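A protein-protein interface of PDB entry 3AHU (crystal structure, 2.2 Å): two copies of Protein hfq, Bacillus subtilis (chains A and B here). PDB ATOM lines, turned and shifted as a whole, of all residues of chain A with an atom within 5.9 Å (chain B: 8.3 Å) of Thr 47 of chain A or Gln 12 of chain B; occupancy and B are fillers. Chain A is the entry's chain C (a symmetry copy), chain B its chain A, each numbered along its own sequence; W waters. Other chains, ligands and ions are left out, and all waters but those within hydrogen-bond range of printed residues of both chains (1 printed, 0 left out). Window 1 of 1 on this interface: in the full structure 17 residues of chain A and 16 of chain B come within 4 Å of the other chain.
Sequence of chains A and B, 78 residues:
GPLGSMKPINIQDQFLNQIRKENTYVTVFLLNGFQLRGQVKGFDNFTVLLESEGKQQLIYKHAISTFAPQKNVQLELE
O of Asp 44 of chain B sits at hydrogen-bond distance from NZ of Lys 61 of chain B (2.9 Å).
The backbone NH of Val 48 of chain A lies within hydrogen-bond range of the backbone carbonyl oxygen of Ile 59 of chain A, 2.9 Å away.
OD1 of Asp 44 of chain A sits at hydrogen-bond distance from OG1 of Thr 47 of chain A.
The side-chain amide oxygen (OE1) of Gln 12 of chain B lies within hydrogen-bond range of the side-chain amino group (NZ) of Lys 61 of chain B.
The backbone carbonyl oxygen (O) of Phe 46 of chain A lies within hydrogen-bond range of the backbone NH (N) of Lys 61 of chain A, at 2.8 Å.
NZ of Lys 61 of chain A lies within hydrogen-bond range of O of Asp 44 of chain A.
The backbone carbonyl oxygen (O) of Leu 58 of chain A is in hydrogen-bond range of the backbone NH (N) of Phe 67 of chain B, at 2.8 Å.
The backbone NH (N) of Ile 11 of chain B sits at hydrogen-bond distance from the side-chain carboxylate (OD2) of Asp 44 of chain A.
OE1 of Gln 12 of chain B sits at hydrogen-bond distance from OH of Tyr 60 of chain A (2.9 Å).
The side-chain carboxylate of Asp 44 of chain A sits close to the side-chain amide oxygen of Asn 10 of chain B, at 2.7 Å.
The backbone NH (N) of Gln 12 of chain B sits at hydrogen-bond distance from the side-chain carboxylate (OD2) of Asp 44 of chain A (3.0 Å).
The backbone NH (N) of Tyr 60 of chain A sits at hydrogen-bond distance from the backbone carbonyl oxygen (O) of Ser 65 of chain B (3.0 Å).
Printed residues of chain B within 4 Å of Gly 42 of chain A: Ile 11.
Of the printed residues of chain B, Phe 43 of chain A touches Ile 11.
Printed residues of chain B within 4 Å of Phe 46 of chain A: Gln 12.
Printed residues of chain B within 4 Å of Thr 47 of chain A: Gln 12 (3.8 Å).
Of the printed residues of chain A, Ser 65 of chain B touches Ile 59 and Tyr 60.
The nearest residue of chain B that does not touch Thr 47 of chain A is Ile 11 of chain B (4.5 Å).
Among the printed residues, pairs that only touch across the chains: Ile 59 of chain A with Ser 65 of chain B (3.2 Å), Phe 43 of chain A with Ile 11 of chain B (3.3 Å), Tyr 60 of chain A with Phe 67 of chain B (3.4 Å), Tyr 60 of chain A with Lys 61 of chain B (3.5 Å), Gly 42 of chain A with Ile 11 of chain B (3.5 Å), Leu 58 of chain A with Phe 15 of chain B (3.6 Å), Tyr 60 of chain A with Ile 64 of chain B (3.7 Å), Thr 47 of chain A with Gln 12 of chain B (3.8 Å), Leu 49 of chain A with Leu 75 of chain B (3.8 Å), Leu 58 of chain A with Ile 11 of chain B (3.8 Å), Leu 49 of chain A with Phe 15 of chain B (3.9 Å) and Phe 46 of chain A with Gln 12 of chain B (3.9 Å).
Positions printed for both chains: 43, 44, 45, 46, 47, 48 and 61.
Of the 18 pairs that touch across the chains among the printed residues, none has its exchanged pair printed and touching as well.
Of the 12 printed residues of chain A, 9 touch a printed residue of chain B.
Hydrophobic or aromatic side chains of chain A that line the printed part of chain B: Phe 46, Leu 49, Leu 58, Ile 59 and Tyr 60.
Hydrophobic or aromatic side chains of chain B within 4 Å of the printed part of chain A: Ile 11, Phe 15, Ile 64, Phe 67 and Leu 75.
Among the printed residues, no Asp or Glu carboxylate lies within 4 Å of a Lys or Arg side-chain nitrogen of the other chain.
Water W1 lies within hydrogen-bond range of the side-chain carboxylate (OD2) of Asp 44 of chain A (2.6 Å), the side-chain amide oxygen (OD1) of Asn 10 of chain B (2.8 Å) and the side-chain amide nitrogen (NE2) of Gln 12 of chain B (3.4 Å).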
ATOM      1  N   GLY A  42      -1.894  13.985 -24.653  1.00  0.00           N
ATOM      2  CA  GLY A  42      -0.809  14.055 -25.708  1.00  0.00           C
ATOM      3  C   GLY A  42      -0.076  12.716 -25.817  1.00  0.00           C
ATOM      4  O   GLY A  42      -0.271  11.828 -24.975  1.00  0.00           O
ATOM      5  N   PHE A  43       0.767  12.568 -26.839  1.00  0.00           N
ATOM      6  CA  PHE A  43       1.506  11.354 -27.021  1.00  0.00           C
ATOM      7  C   PHE A  43       2.669  11.723 -27.968  1.00  0.00           C
ATOM      8  O   PHE A  43       2.727  12.840 -28.567  1.00  0.00           O
ATOM      9  CB  PHE A  43       0.552  10.224 -27.493  1.00  0.00           C
ATOM     10  CG  PHE A  43      -0.087  10.486 -28.845  1.00  0.00           C
ATOM     11  CD1 PHE A  43       0.467   9.936 -29.996  1.00  0.00           C
ATOM     12  CD2 PHE A  43      -1.136  11.405 -28.977  1.00  0.00           C
ATOM     13  CE1 PHE A  43      -0.054  10.196 -31.200  1.00  0.00           C
ATOM     14  CE2 PHE A  43      -1.699  11.671 -30.198  1.00  0.00           C
ATOM     15  CZ  PHE A  43      -1.175  11.097 -31.297  1.00  0.00           C
ATOM     16  N   ASP A  44       3.715  10.921 -27.943  1.00  0.00           N
ATOM     17  CA  ASP A  44       4.719  10.957 -28.943  1.00  0.00           C
ATOM     18  C   ASP A  44       5.070   9.514 -29.328  1.00  0.00           C
ATOM     19  O   ASP A  44       4.290   8.559 -29.055  1.00  0.00           O
ATOM     20  CB  ASP A  44       5.887  11.862 -28.592  1.00  0.00           C
ATOM     21  CG  ASP A  44       6.663  11.399 -27.300  1.00  0.00           C
ATOM     22  OD1 ASP A  44       6.509  10.276 -26.870  1.00  0.00           O
ATOM     23  OD2 ASP A  44       7.502  12.145 -26.773  1.00  0.00           O
ATOM     24  N   ASN A  45       6.154   9.372 -30.071  1.00  0.00           N
ATOM     25  CA  ASN A  45       6.691   8.071 -30.487  1.00  0.00           C
ATOM     26  C   ASN A  45       6.808   6.979 -29.413  1.00  0.00           C
ATOM     27  O   ASN A  45       6.423   5.770 -29.623  1.00  0.00           O
ATOM     28  CB  ASN A  45       7.981   8.271 -31.248  1.00  0.00           C
ATOM     29  CG  ASN A  45       7.705   8.660 -32.739  1.00  0.00           C
ATOM     30  OD1 ASN A  45       6.754   8.194 -33.337  1.00  0.00           O
ATOM     31  ND2 ASN A  45       8.580   9.406 -33.325  1.00  0.00           N
ATOM     32  N   PHE A  46       7.197   7.404 -28.243  1.00  0.00           N
ATOM     33  CA  PHE A  46       7.600   6.501 -27.176  1.00  0.00           C
ATOM     34  C   PHE A  46       6.633   6.495 -25.927  1.00  0.00           C
ATOM     35  O   PHE A  46       6.716   5.587 -25.134  1.00  0.00           O
ATOM     36  CB  PHE A  46       8.953   6.944 -26.736  1.00  0.00           C
ATOM     37  CG  PHE A  46      10.077   6.547 -27.705  1.00  0.00           C
ATOM     38  CD1 PHE A  46      10.896   7.517 -28.255  1.00  0.00           C
ATOM     39  CD2 PHE A  46      10.328   5.202 -28.021  1.00  0.00           C
ATOM     40  CE1 PHE A  46      11.962   7.131 -29.082  1.00  0.00           C
ATOM     41  CE2 PHE A  46      11.345   4.852 -28.830  1.00  0.00           C
ATOM     42  CZ  PHE A  46      12.182   5.891 -29.361  1.00  0.00           C
ATOM     43  N   THR A  47       5.755   7.520 -25.770  1.00  0.00           N
ATOM     44  CA  THR A  47       5.121   7.857 -24.457  1.00  0.00           C
ATOM     45  C   THR A  47       3.683   8.410 -24.672  1.00  0.00           C
ATOM     46  O   THR A  47       3.373   8.927 -25.752  1.00  0.00           O
ATOM     47  CB  THR A  47       5.933   8.947 -23.584  1.00  0.00           C
ATOM     48  OG1 THR A  47       5.994  10.225 -24.225  1.00  0.00           O
ATOM     49  CG2 THR A  47       7.391   8.534 -23.072  1.00  0.00           C
ATOM     50  N   VAL A  48       2.793   8.178 -23.695  1.00  0.00           N
ATOM     51  CA  VAL A  48       1.426   8.647 -23.661  1.00  0.00           C
ATOM     52  C   VAL A  48       1.291   9.455 -22.297  1.00  0.00           C
ATOM     53  O   VAL A  48       1.473   8.908 -21.242  1.00  0.00           O
ATOM     54  CB  VAL A  48       0.464   7.519 -23.754  1.00  0.00           C
ATOM     55  CG1 VAL A  48      -1.000   8.026 -23.732  1.00  0.00           C
ATOM     56  CG2 VAL A  48       0.588   6.690 -25.076  1.00  0.00           C
ATOM     57  N   LEU A  49       1.116  10.768 -22.374  1.00  0.00           N
ATOM     58  CA  LEU A  49       0.700  11.620 -21.248  1.00  0.00           C
ATOM     59  C   LEU A  49      -0.808  11.364 -20.932  1.00  0.00           C
ATOM     60  O   LEU A  49      -1.698  11.610 -21.730  1.00  0.00           O
ATOM     61  CB  LEU A  49       1.088  13.074 -21.521  1.00  0.00           C
ATOM     62  CG  LEU A  49       0.873  14.099 -20.399  1.00  0.00           C
ATOM     63  CD1 LEU A  49       1.790  13.992 -19.194  1.00  0.00           C
ATOM     64  CD2 LEU A  49       1.036  15.461 -21.032  1.00  0.00           C
ATOM     65  N   LEU A  58       3.337  10.278 -17.106  1.00  0.00           N
ATOM     66  CA  LEU A  58       4.003   9.986 -18.378  1.00  0.00           C
ATOM     67  C   LEU A  58       4.215   8.436 -18.363  1.00  0.00           C
ATOM     68  O   LEU A  58       4.935   7.974 -17.558  1.00  0.00           O
ATOM     69  CB  LEU A  58       5.280  10.828 -18.529  1.00  0.00           C
ATOM     70  CG  LEU A  58       5.970  10.687 -19.920  1.00  0.00           C
ATOM     71  CD1 LEU A  58       5.225  11.428 -21.037  1.00  0.00           C
ATOM     72  CD2 LEU A  58       7.423  10.988 -19.969  1.00  0.00           C
ATOM     73  N   ILE A  59       3.455   7.680 -19.165  1.00  0.00           N
ATOM     74  CA  ILE A  59       3.591   6.227 -19.448  1.00  0.00           C
ATOM     75  C   ILE A  59       4.449   5.941 -20.774  1.00  0.00           C
ATOM     76  O   ILE A  59       4.058   6.390 -21.859  1.00  0.00           O
ATOM     77  CB  ILE A  59       2.200   5.699 -19.638  1.00  0.00           C
ATOM     78  CG1 ILE A  59       1.201   6.529 -18.754  1.00  0.00           C
ATOM     79  CG2 ILE A  59       2.031   4.038 -19.584  1.00  0.00           C
ATOM     80  CD1 ILE A  59      -0.209   5.961 -18.686  1.00  0.00           C
ATOM     81  N   TYR A  60       5.487   5.147 -20.686  1.00  0.00           N
ATOM     82  CA  TYR A  60       6.109   4.592 -21.857  1.00  0.00           C
ATOM     83  C   TYR A  60       5.172   3.633 -22.623  1.00  0.00           C
ATOM     84  O   TYR A  60       4.577   2.789 -22.041  1.00  0.00           O
ATOM     85  CB  TYR A  60       7.408   3.909 -21.440  1.00  0.00           C
ATOM     86  CG  TYR A  60       8.469   4.902 -21.128  1.00  0.00           C
ATOM     87  CD1 TYR A  60       9.075   5.586 -22.116  1.00  0.00           C
ATOM     88  CD2 TYR A  60       8.819   5.186 -19.863  1.00  0.00           C
ATOM     89  CE1 TYR A  60      10.000   6.509 -21.847  1.00  0.00           C
ATOM     90  CE2 TYR A  60       9.791   6.103 -19.598  1.00  0.00           C
ATOM     91  CZ  TYR A  60      10.345   6.755 -20.602  1.00  0.00           C
ATOM     92  OH  TYR A  60      11.261   7.649 -20.364  1.00  0.00           O
ATOM     93  N   LYS A  61       5.003   3.765 -23.920  1.00  0.00           N
ATOM     94  CA  LYS A  61       4.123   2.702 -24.488  1.00  0.00           C
ATOM     95  C   LYS A  61       4.597   1.302 -24.430  1.00  0.00           C
ATOM     96  O   LYS A  61       3.767   0.346 -24.524  1.00  0.00           O
ATOM     97  CB  LYS A  61       4.007   2.956 -25.969  1.00  0.00           C
ATOM     98  CG  LYS A  61       3.563   4.376 -26.307  1.00  0.00           C
ATOM     99  CD  LYS A  61       3.821   4.591 -27.821  1.00  0.00           C
ATOM    100  CE  LYS A  61       3.268   6.016 -28.096  1.00  0.00           C
ATOM    101  NZ  LYS A  61       3.088   6.119 -29.545  1.00  0.00           N
ATOM    102  N   ASN B  10       7.966  17.013 -28.868  1.00  0.00           N
ATOM    103  CA  ASN B  10       8.388  15.807 -28.085  1.00  0.00           C
ATOM    104  C   ASN B  10       7.899  15.963 -26.677  1.00  0.00           C
ATOM    105  O   ASN B  10       8.372  16.804 -25.954  1.00  0.00           O
ATOM    106  CB  ASN B  10       9.906  15.632 -28.112  1.00  0.00           C
ATOM    107  CG  ASN B  10      10.355  14.170 -27.740  1.00  0.00           C
ATOM    108  OD1 ASN B  10       9.780  13.504 -26.842  1.00  0.00           O
ATOM    109  ND2 ASN B  10      11.371  13.681 -28.450  1.00  0.00           N
ATOM    110  N   ILE B  11       6.874  15.215 -26.288  1.00  0.00           N
ATOM    111  CA  ILE B  11       6.421  15.302 -24.913  1.00  0.00           C
ATOM    112  C   ILE B  11       7.323  14.721 -23.848  1.00  0.00           C
ATOM    113  O   ILE B  11       7.504  15.349 -22.765  1.00  0.00           O
ATOM    114  CB  ILE B  11       5.125  14.653 -24.716  1.00  0.00           C
ATOM    115  CG1 ILE B  11       4.071  15.510 -25.419  1.00  0.00           C
ATOM    116  CG2 ILE B  11       4.898  14.606 -23.157  1.00  0.00           C
ATOM    117  CD1 ILE B  11       2.690  14.877 -25.494  1.00  0.00           C
ATOM    118  N   GLN B  12       7.950  13.586 -24.129  1.00  0.00           N
ATOM    119  CA  GLN B  12       8.823  12.937 -23.174  1.00  0.00           C
ATOM    120  C   GLN B  12       9.917  13.828 -22.714  1.00  0.00           C
ATOM    121  O   GLN B  12      10.218  13.874 -21.563  1.00  0.00           O
ATOM    122  CB  GLN B  12       9.456  11.644 -23.709  1.00  0.00           C
ATOM    123  CG  GLN B  12      10.369  10.975 -22.681  1.00  0.00           C
ATOM    124  CD  GLN B  12      11.219   9.820 -23.190  1.00  0.00           C
ATOM    125  OE1 GLN B  12      12.099   9.372 -22.519  1.00  0.00           O
ATOM    126  NE2 GLN B  12      10.962   9.374 -24.368  1.00  0.00           N
ATOM    127  N   ASP B  13      10.563  14.500 -23.630  1.00  0.00           N
ATOM    128  CA  ASP B  13      11.719  15.261 -23.259  1.00  0.00           C
ATOM    129  C   ASP B  13      11.316  16.547 -22.571  1.00  0.00           C
ATOM    130  O   ASP B  13      12.028  17.036 -21.761  1.00  0.00           O
ATOM    131  CB  ASP B  13      12.586  15.579 -24.453  1.00  0.00           C
ATOM    132  CG  ASP B  13      13.243  14.375 -25.057  1.00  0.00           C
ATOM    133  OD1 ASP B  13      13.487  13.381 -24.399  1.00  0.00           O
ATOM    134  OD2 ASP B  13      13.524  14.460 -26.227  1.00  0.00           O
ATOM    135  N   GLN B  14      10.168  17.082 -22.916  1.00  0.00           N
ATOM    136  CA  GLN B  14       9.674  18.251 -22.270  1.00  0.00           C
ATOM    137  C   GLN B  14       9.311  17.860 -20.892  1.00  0.00           C
ATOM    138  O   GLN B  14       9.781  18.414 -19.953  1.00  0.00           O
ATOM    139  CB  GLN B  14       8.381  18.662 -22.894  1.00  0.00           C
ATOM    140  CG  GLN B  14       8.447  19.397 -24.136  1.00  0.00           C
ATOM    141  CD  GLN B  14       7.087  19.777 -24.527  1.00  0.00           C
ATOM    142  OE1 GLN B  14       6.536  20.706 -23.992  1.00  0.00           O
ATOM    143  NE2 GLN B  14       6.503  19.033 -25.419  1.00  0.00           N
ATOM    144  N   PHE B  15       8.414  16.907 -20.796  1.00  0.00           N
ATOM    145  CA  PHE B  15       7.961  16.405 -19.510  1.00  0.00           C
ATOM    146  C   PHE B  15       9.073  16.141 -18.518  1.00  0.00           C
ATOM    147  O   PHE B  15       8.934  16.490 -17.309  1.00  0.00           O
ATOM    148  CB  PHE B  15       7.100  15.188 -19.672  1.00  0.00           C
ATOM    149  CG  PHE B  15       6.722  14.562 -18.389  1.00  0.00           C
ATOM    150  CD1 PHE B  15       5.422  14.730 -17.887  1.00  0.00           C
ATOM    151  CD2 PHE B  15       7.632  13.735 -17.695  1.00  0.00           C
ATOM    152  CE1 PHE B  15       5.038  14.186 -16.702  1.00  0.00           C
ATOM    153  CE2 PHE B  15       7.264  13.166 -16.468  1.00  0.00           C
ATOM    154  CZ  PHE B  15       5.937  13.375 -15.980  1.00  0.00           C
ATOM    155  N   LEU B  16      10.158  15.572 -19.037  1.00  0.00           N
ATOM    156  CA  LEU B  16      11.265  15.138 -18.283  1.00  0.00           C
ATOM    157  C   LEU B  16      12.292  16.237 -18.065  1.00  0.00           C
ATOM    158  O   LEU B  16      12.959  16.294 -17.008  1.00  0.00           O
ATOM    159  CB  LEU B  16      11.900  13.877 -18.930  1.00  0.00           C
ATOM    160  CG  LEU B  16      11.448  12.409 -18.683  1.00  0.00           C
ATOM    161  CD1 LEU B  16      12.474  11.434 -19.457  1.00  0.00           C
ATOM    162  CD2 LEU B  16      11.767  12.106 -17.297  1.00  0.00           C
ATOM    163  N   ASN B  17      12.460  17.129 -19.024  1.00  0.00           N
ATOM    164  CA  ASN B  17      13.306  18.247 -18.654  1.00  0.00           C
ATOM    165  C   ASN B  17      12.636  19.228 -17.624  1.00  0.00           C
ATOM    166  O   ASN B  17      13.316  19.714 -16.705  1.00  0.00           O
ATOM    167  CB  ASN B  17      14.037  18.948 -19.818  1.00  0.00           C
ATOM    168  CG  ASN B  17      15.479  19.281 -19.436  1.00  0.00           C
ATOM    169  OD1 ASN B  17      15.729  19.657 -18.283  1.00  0.00           O
ATOM    170  ND2 ASN B  17      16.439  19.038 -20.339  1.00  0.00           N
ATOM    171  N   GLN B  18      11.318  19.411 -17.743  1.00  0.00           N
ATOM    172  CA  GLN B  18      10.525  20.206 -16.782  1.00  0.00           C
ATOM    173  C   GLN B  18      10.541  19.666 -15.343  1.00  0.00           C
ATOM    174  O   GLN B  18      10.481  20.462 -14.444  1.00  0.00           O
ATOM    175  CB  GLN B  18       9.064  20.370 -17.189  1.00  0.00           C
ATOM    176  CG  GLN B  18       8.642  21.804 -17.613  1.00  0.00           C
ATOM    177  CD  GLN B  18       8.834  22.103 -19.124  1.00  0.00           C
ATOM    178  OE1 GLN B  18       9.809  21.629 -19.772  1.00  0.00           O
ATOM    179  NE2 GLN B  18       7.923  22.938 -19.686  1.00  0.00           N
ATOM    180  N   ILE B  19      10.612  18.344 -15.133  1.00  0.00           N
ATOM    181  CA  ILE B  19      10.636  17.780 -13.785  1.00  0.00           C
ATOM    182  C   ILE B  19      12.066  17.772 -13.220  1.00  0.00           C
ATOM    183  O   ILE B  19      12.318  17.866 -12.012  1.00  0.00           O
ATOM    184  CB  ILE B  19       9.836  16.417 -13.680  1.00  0.00           C
ATOM    185  CG1 ILE B  19      10.640  15.207 -14.127  1.00  0.00           C
ATOM    186  CG2 ILE B  19       8.645  16.495 -14.541  1.00  0.00           C
ATOM    187  CD1 ILE B  19      10.123  13.859 -13.613  1.00  0.00           C
ATOM    188  N   PHE B  43      18.861  12.791 -18.095  1.00  0.00           N
ATOM    189  CA  PHE B  43      18.434  11.688 -18.897  1.00  0.00           C
ATOM    190  C   PHE B  43      19.153  11.663 -20.232  1.00  0.00           C
ATOM    191  O   PHE B  43      19.757  12.604 -20.616  1.00  0.00           O
ATOM    192  CB  PHE B  43      16.935  11.686 -19.068  1.00  0.00           C
ATOM    193  CG  PHE B  43      16.366  12.979 -19.509  1.00  0.00           C
ATOM    194  CD1 PHE B  43      15.869  13.119 -20.772  1.00  0.00           C
ATOM    195  CD2 PHE B  43      16.289  14.035 -18.657  1.00  0.00           C
ATOM    196  CE1 PHE B  43      15.338  14.280 -21.171  1.00  0.00           C
ATOM    197  CE2 PHE B  43      15.746  15.205 -19.058  1.00  0.00           C
ATOM    198  CZ  PHE B  43      15.272  15.328 -20.313  1.00  0.00           C
ATOM    199  N   ASP B  44      19.124  10.533 -20.896  1.00  0.00           N
ATOM    200  CA  ASP B  44      19.532  10.441 -22.270  1.00  0.00           C
ATOM    201  C   ASP B  44      18.475   9.653 -23.003  1.00  0.00           C
ATOM    202  O   ASP B  44      17.404   9.544 -22.506  1.00  0.00           O
ATOM    203  CB  ASP B  44      20.960   9.933 -22.452  1.00  0.00           C
ATOM    204  CG  ASP B  44      21.221   8.599 -21.842  1.00  0.00           C
ATOM    205  OD1 ASP B  44      20.349   7.798 -21.618  1.00  0.00           O
ATOM    206  OD2 ASP B  44      22.355   8.332 -21.613  1.00  0.00           O
ATOM    207  N   ASN B  45      18.758   9.147 -24.189  1.00  0.00           N
ATOM    208  CA  ASN B  45      17.729   8.478 -24.964  1.00  0.00           C
ATOM    209  C   ASN B  45      17.386   7.128 -24.405  1.00  0.00           C
ATOM    210  O   ASN B  45      16.372   6.603 -24.675  1.00  0.00           O
ATOM    211  CB  ASN B  45      18.092   8.361 -26.447  1.00  0.00           C
ATOM    212  CG  ASN B  45      18.066   9.689 -27.183  1.00  0.00           C
ATOM    213  OD1 ASN B  45      17.419  10.654 -26.793  1.00  0.00           O
ATOM    214  ND2 ASN B  45      18.785   9.728 -28.272  1.00  0.00           N
ATOM    215  N   PHE B  46      18.244   6.561 -23.593  1.00  0.00           N
ATOM    216  CA  PHE B  46      18.045   5.247 -23.017  1.00  0.00           C
ATOM    217  C   PHE B  46      17.860   5.160 -21.483  1.00  0.00           C
ATOM    218  O   PHE B  46      17.343   4.212 -20.996  1.00  0.00           O
ATOM    219  CB  PHE B  46      19.207   4.358 -23.415  1.00  0.00           C
ATOM    220  CG  PHE B  46      19.276   4.060 -24.870  1.00  0.00           C
ATOM    221  CD1 PHE B  46      20.256   4.593 -25.641  1.00  0.00           C
ATOM    222  CD2 PHE B  46      18.356   3.246 -25.462  1.00  0.00           C
ATOM    223  CE1 PHE B  46      20.306   4.322 -26.968  1.00  0.00           C
ATOM    224  CE2 PHE B  46      18.420   2.985 -26.765  1.00  0.00           C
ATOM    225  CZ  PHE B  46      19.391   3.514 -27.519  1.00  0.00           C
ATOM    226  N   THR B  47      18.333   6.146 -20.754  1.00  0.00           N
ATOM    227  CA  THR B  47      18.401   6.143 -19.306  1.00  0.00           C
ATOM    228  C   THR B  47      17.822   7.464 -18.657  1.00  0.00           C
ATOM    229  O   THR B  47      17.727   8.530 -19.340  1.00  0.00           O
ATOM    230  CB  THR B  47      19.812   5.818 -18.783  1.00  0.00           C
ATOM    231  OG1 THR B  47      20.790   6.915 -18.922  1.00  0.00           O
ATOM    232  CG2 THR B  47      20.397   4.472 -19.267  1.00  0.00           C
ATOM    233  N   VAL B  48      17.376   7.313 -17.372  1.00  0.00           N
ATOM    234  CA  VAL B  48      17.008   8.372 -16.397  1.00  0.00           C
ATOM    235  C   VAL B  48      17.986   8.279 -15.136  1.00  0.00           C
ATOM    236  O   VAL B  48      18.200   7.210 -14.550  1.00  0.00           O
ATOM    237  CB  VAL B  48      15.480   8.319 -16.071  1.00  0.00           C
ATOM    238  CG1 VAL B  48      14.992   9.479 -15.146  1.00  0.00           C
ATOM    239  CG2 VAL B  48      14.530   8.372 -17.376  1.00  0.00           C
ATOM    240  N   LYS B  61      15.231   3.347 -19.390  1.00  0.00           N
ATOM    241  CA  LYS B  61      13.801   3.629 -19.730  1.00  0.00           C
ATOM    242  C   LYS B  61      13.043   2.398 -20.059  1.00  0.00           C
ATOM    243  O   LYS B  61      11.825   2.278 -19.781  1.00  0.00           O
ATOM    244  CB  LYS B  61      13.732   4.594 -20.921  1.00  0.00           C
ATOM    245  CG  LYS B  61      14.401   5.890 -20.595  1.00  0.00           C
ATOM    246  CD  LYS B  61      14.276   6.729 -21.924  1.00  0.00           C
ATOM    247  CE  LYS B  61      14.735   8.134 -21.641  1.00  0.00           C
ATOM    248  NZ  LYS B  61      14.604   8.902 -22.981  1.00  0.00           N
ATOM    249  N   ILE B  64      11.052   1.209 -17.052  1.00  0.00           N
ATOM    250  CA  ILE B  64      10.072   2.153 -16.503  1.00  0.00           C
ATOM    251  C   ILE B  64       8.761   1.977 -17.146  1.00  0.00           C
ATOM    252  O   ILE B  64       8.649   1.744 -18.390  1.00  0.00           O
ATOM    253  CB  ILE B  64      10.533   3.573 -16.688  1.00  0.00           C
ATOM    254  CG1 ILE B  64      11.920   3.732 -16.083  1.00  0.00           C
ATOM    255  CG2 ILE B  64       9.400   4.673 -16.082  1.00  0.00           C
ATOM    256  CD1 ILE B  64      12.591   5.065 -16.380  1.00  0.00           C
ATOM    257  N   SER B  65       7.735   1.995 -16.311  1.00  0.00           N
ATOM    258  CA  SER B  65       6.380   2.005 -16.740  1.00  0.00           C
ATOM    259  C   SER B  65       5.779   3.501 -16.864  1.00  0.00           C
ATOM    260  O   SER B  65       5.323   3.959 -17.989  1.00  0.00           O
ATOM    261  CB  SER B  65       5.653   1.326 -15.681  1.00  0.00           C
ATOM    262  OG  SER B  65       4.281   1.476 -15.850  1.00  0.00           O
ATOM    263  N   PHE B  67       5.952   7.692 -14.927  1.00  0.00           N
ATOM    264  CA  PHE B  67       6.504   8.710 -14.023  1.00  0.00           C
ATOM    265  C   PHE B  67       5.269   9.428 -13.460  1.00  0.00           C
ATOM    266  O   PHE B  67       4.529  10.005 -14.240  1.00  0.00           O
ATOM    267  CB  PHE B  67       7.384   9.807 -14.692  1.00  0.00           C
ATOM    268  CG  PHE B  67       8.687   9.300 -15.264  1.00  0.00           C
ATOM    269  CD1 PHE B  67       8.745   8.881 -16.561  1.00  0.00           C
ATOM    270  CD2 PHE B  67       9.820   9.263 -14.523  1.00  0.00           C
ATOM    271  CE1 PHE B  67       9.930   8.393 -17.103  1.00  0.00           C
ATOM    272  CE2 PHE B  67      11.003   8.742 -15.056  1.00  0.00           C
ATOM    273  CZ  PHE B  67      11.048   8.327 -16.387  1.00  0.00           C
ATOM    274  N   VAL B  73       2.874  19.090 -14.759  1.00  0.00           N
ATOM    275  CA  VAL B  73       3.966  19.824 -15.497  1.00  0.00           C
ATOM    276  C   VAL B  73       3.383  20.688 -16.609  1.00  0.00           C
ATOM    277  O   VAL B  73       2.350  20.319 -17.168  1.00  0.00           O
ATOM    278  CB  VAL B  73       5.019  18.800 -16.066  1.00  0.00           C
ATOM    279  CG1 VAL B  73       5.755  19.340 -17.289  1.00  0.00           C
ATOM    280  CG2 VAL B  73       5.986  18.399 -14.962  1.00  0.00           C
ATOM    281  N   LEU B  75       3.575  21.976 -20.372  1.00  0.00           N
ATOM    282  CA  LEU B  75       4.138  21.628 -21.701  1.00  0.00           C
ATOM    283  C   LEU B  75       3.203  21.874 -22.935  1.00  0.00           C
ATOM    284  O   LEU B  75       1.981  21.771 -22.699  1.00  0.00           O
ATOM    285  CB  LEU B  75       4.694  20.169 -21.666  1.00  0.00           C
ATOM    286  CG  LEU B  75       3.807  19.050 -21.132  1.00  0.00           C
ATOM    287  CD1 LEU B  75       2.901  18.561 -22.249  1.00  0.00           C
ATOM    288  CD2 LEU B  75       4.679  17.944 -20.615  1.00  0.00           C
HETATM  289  O   HOH W   1       9.633  10.686 -27.165  1.00  0.00           O
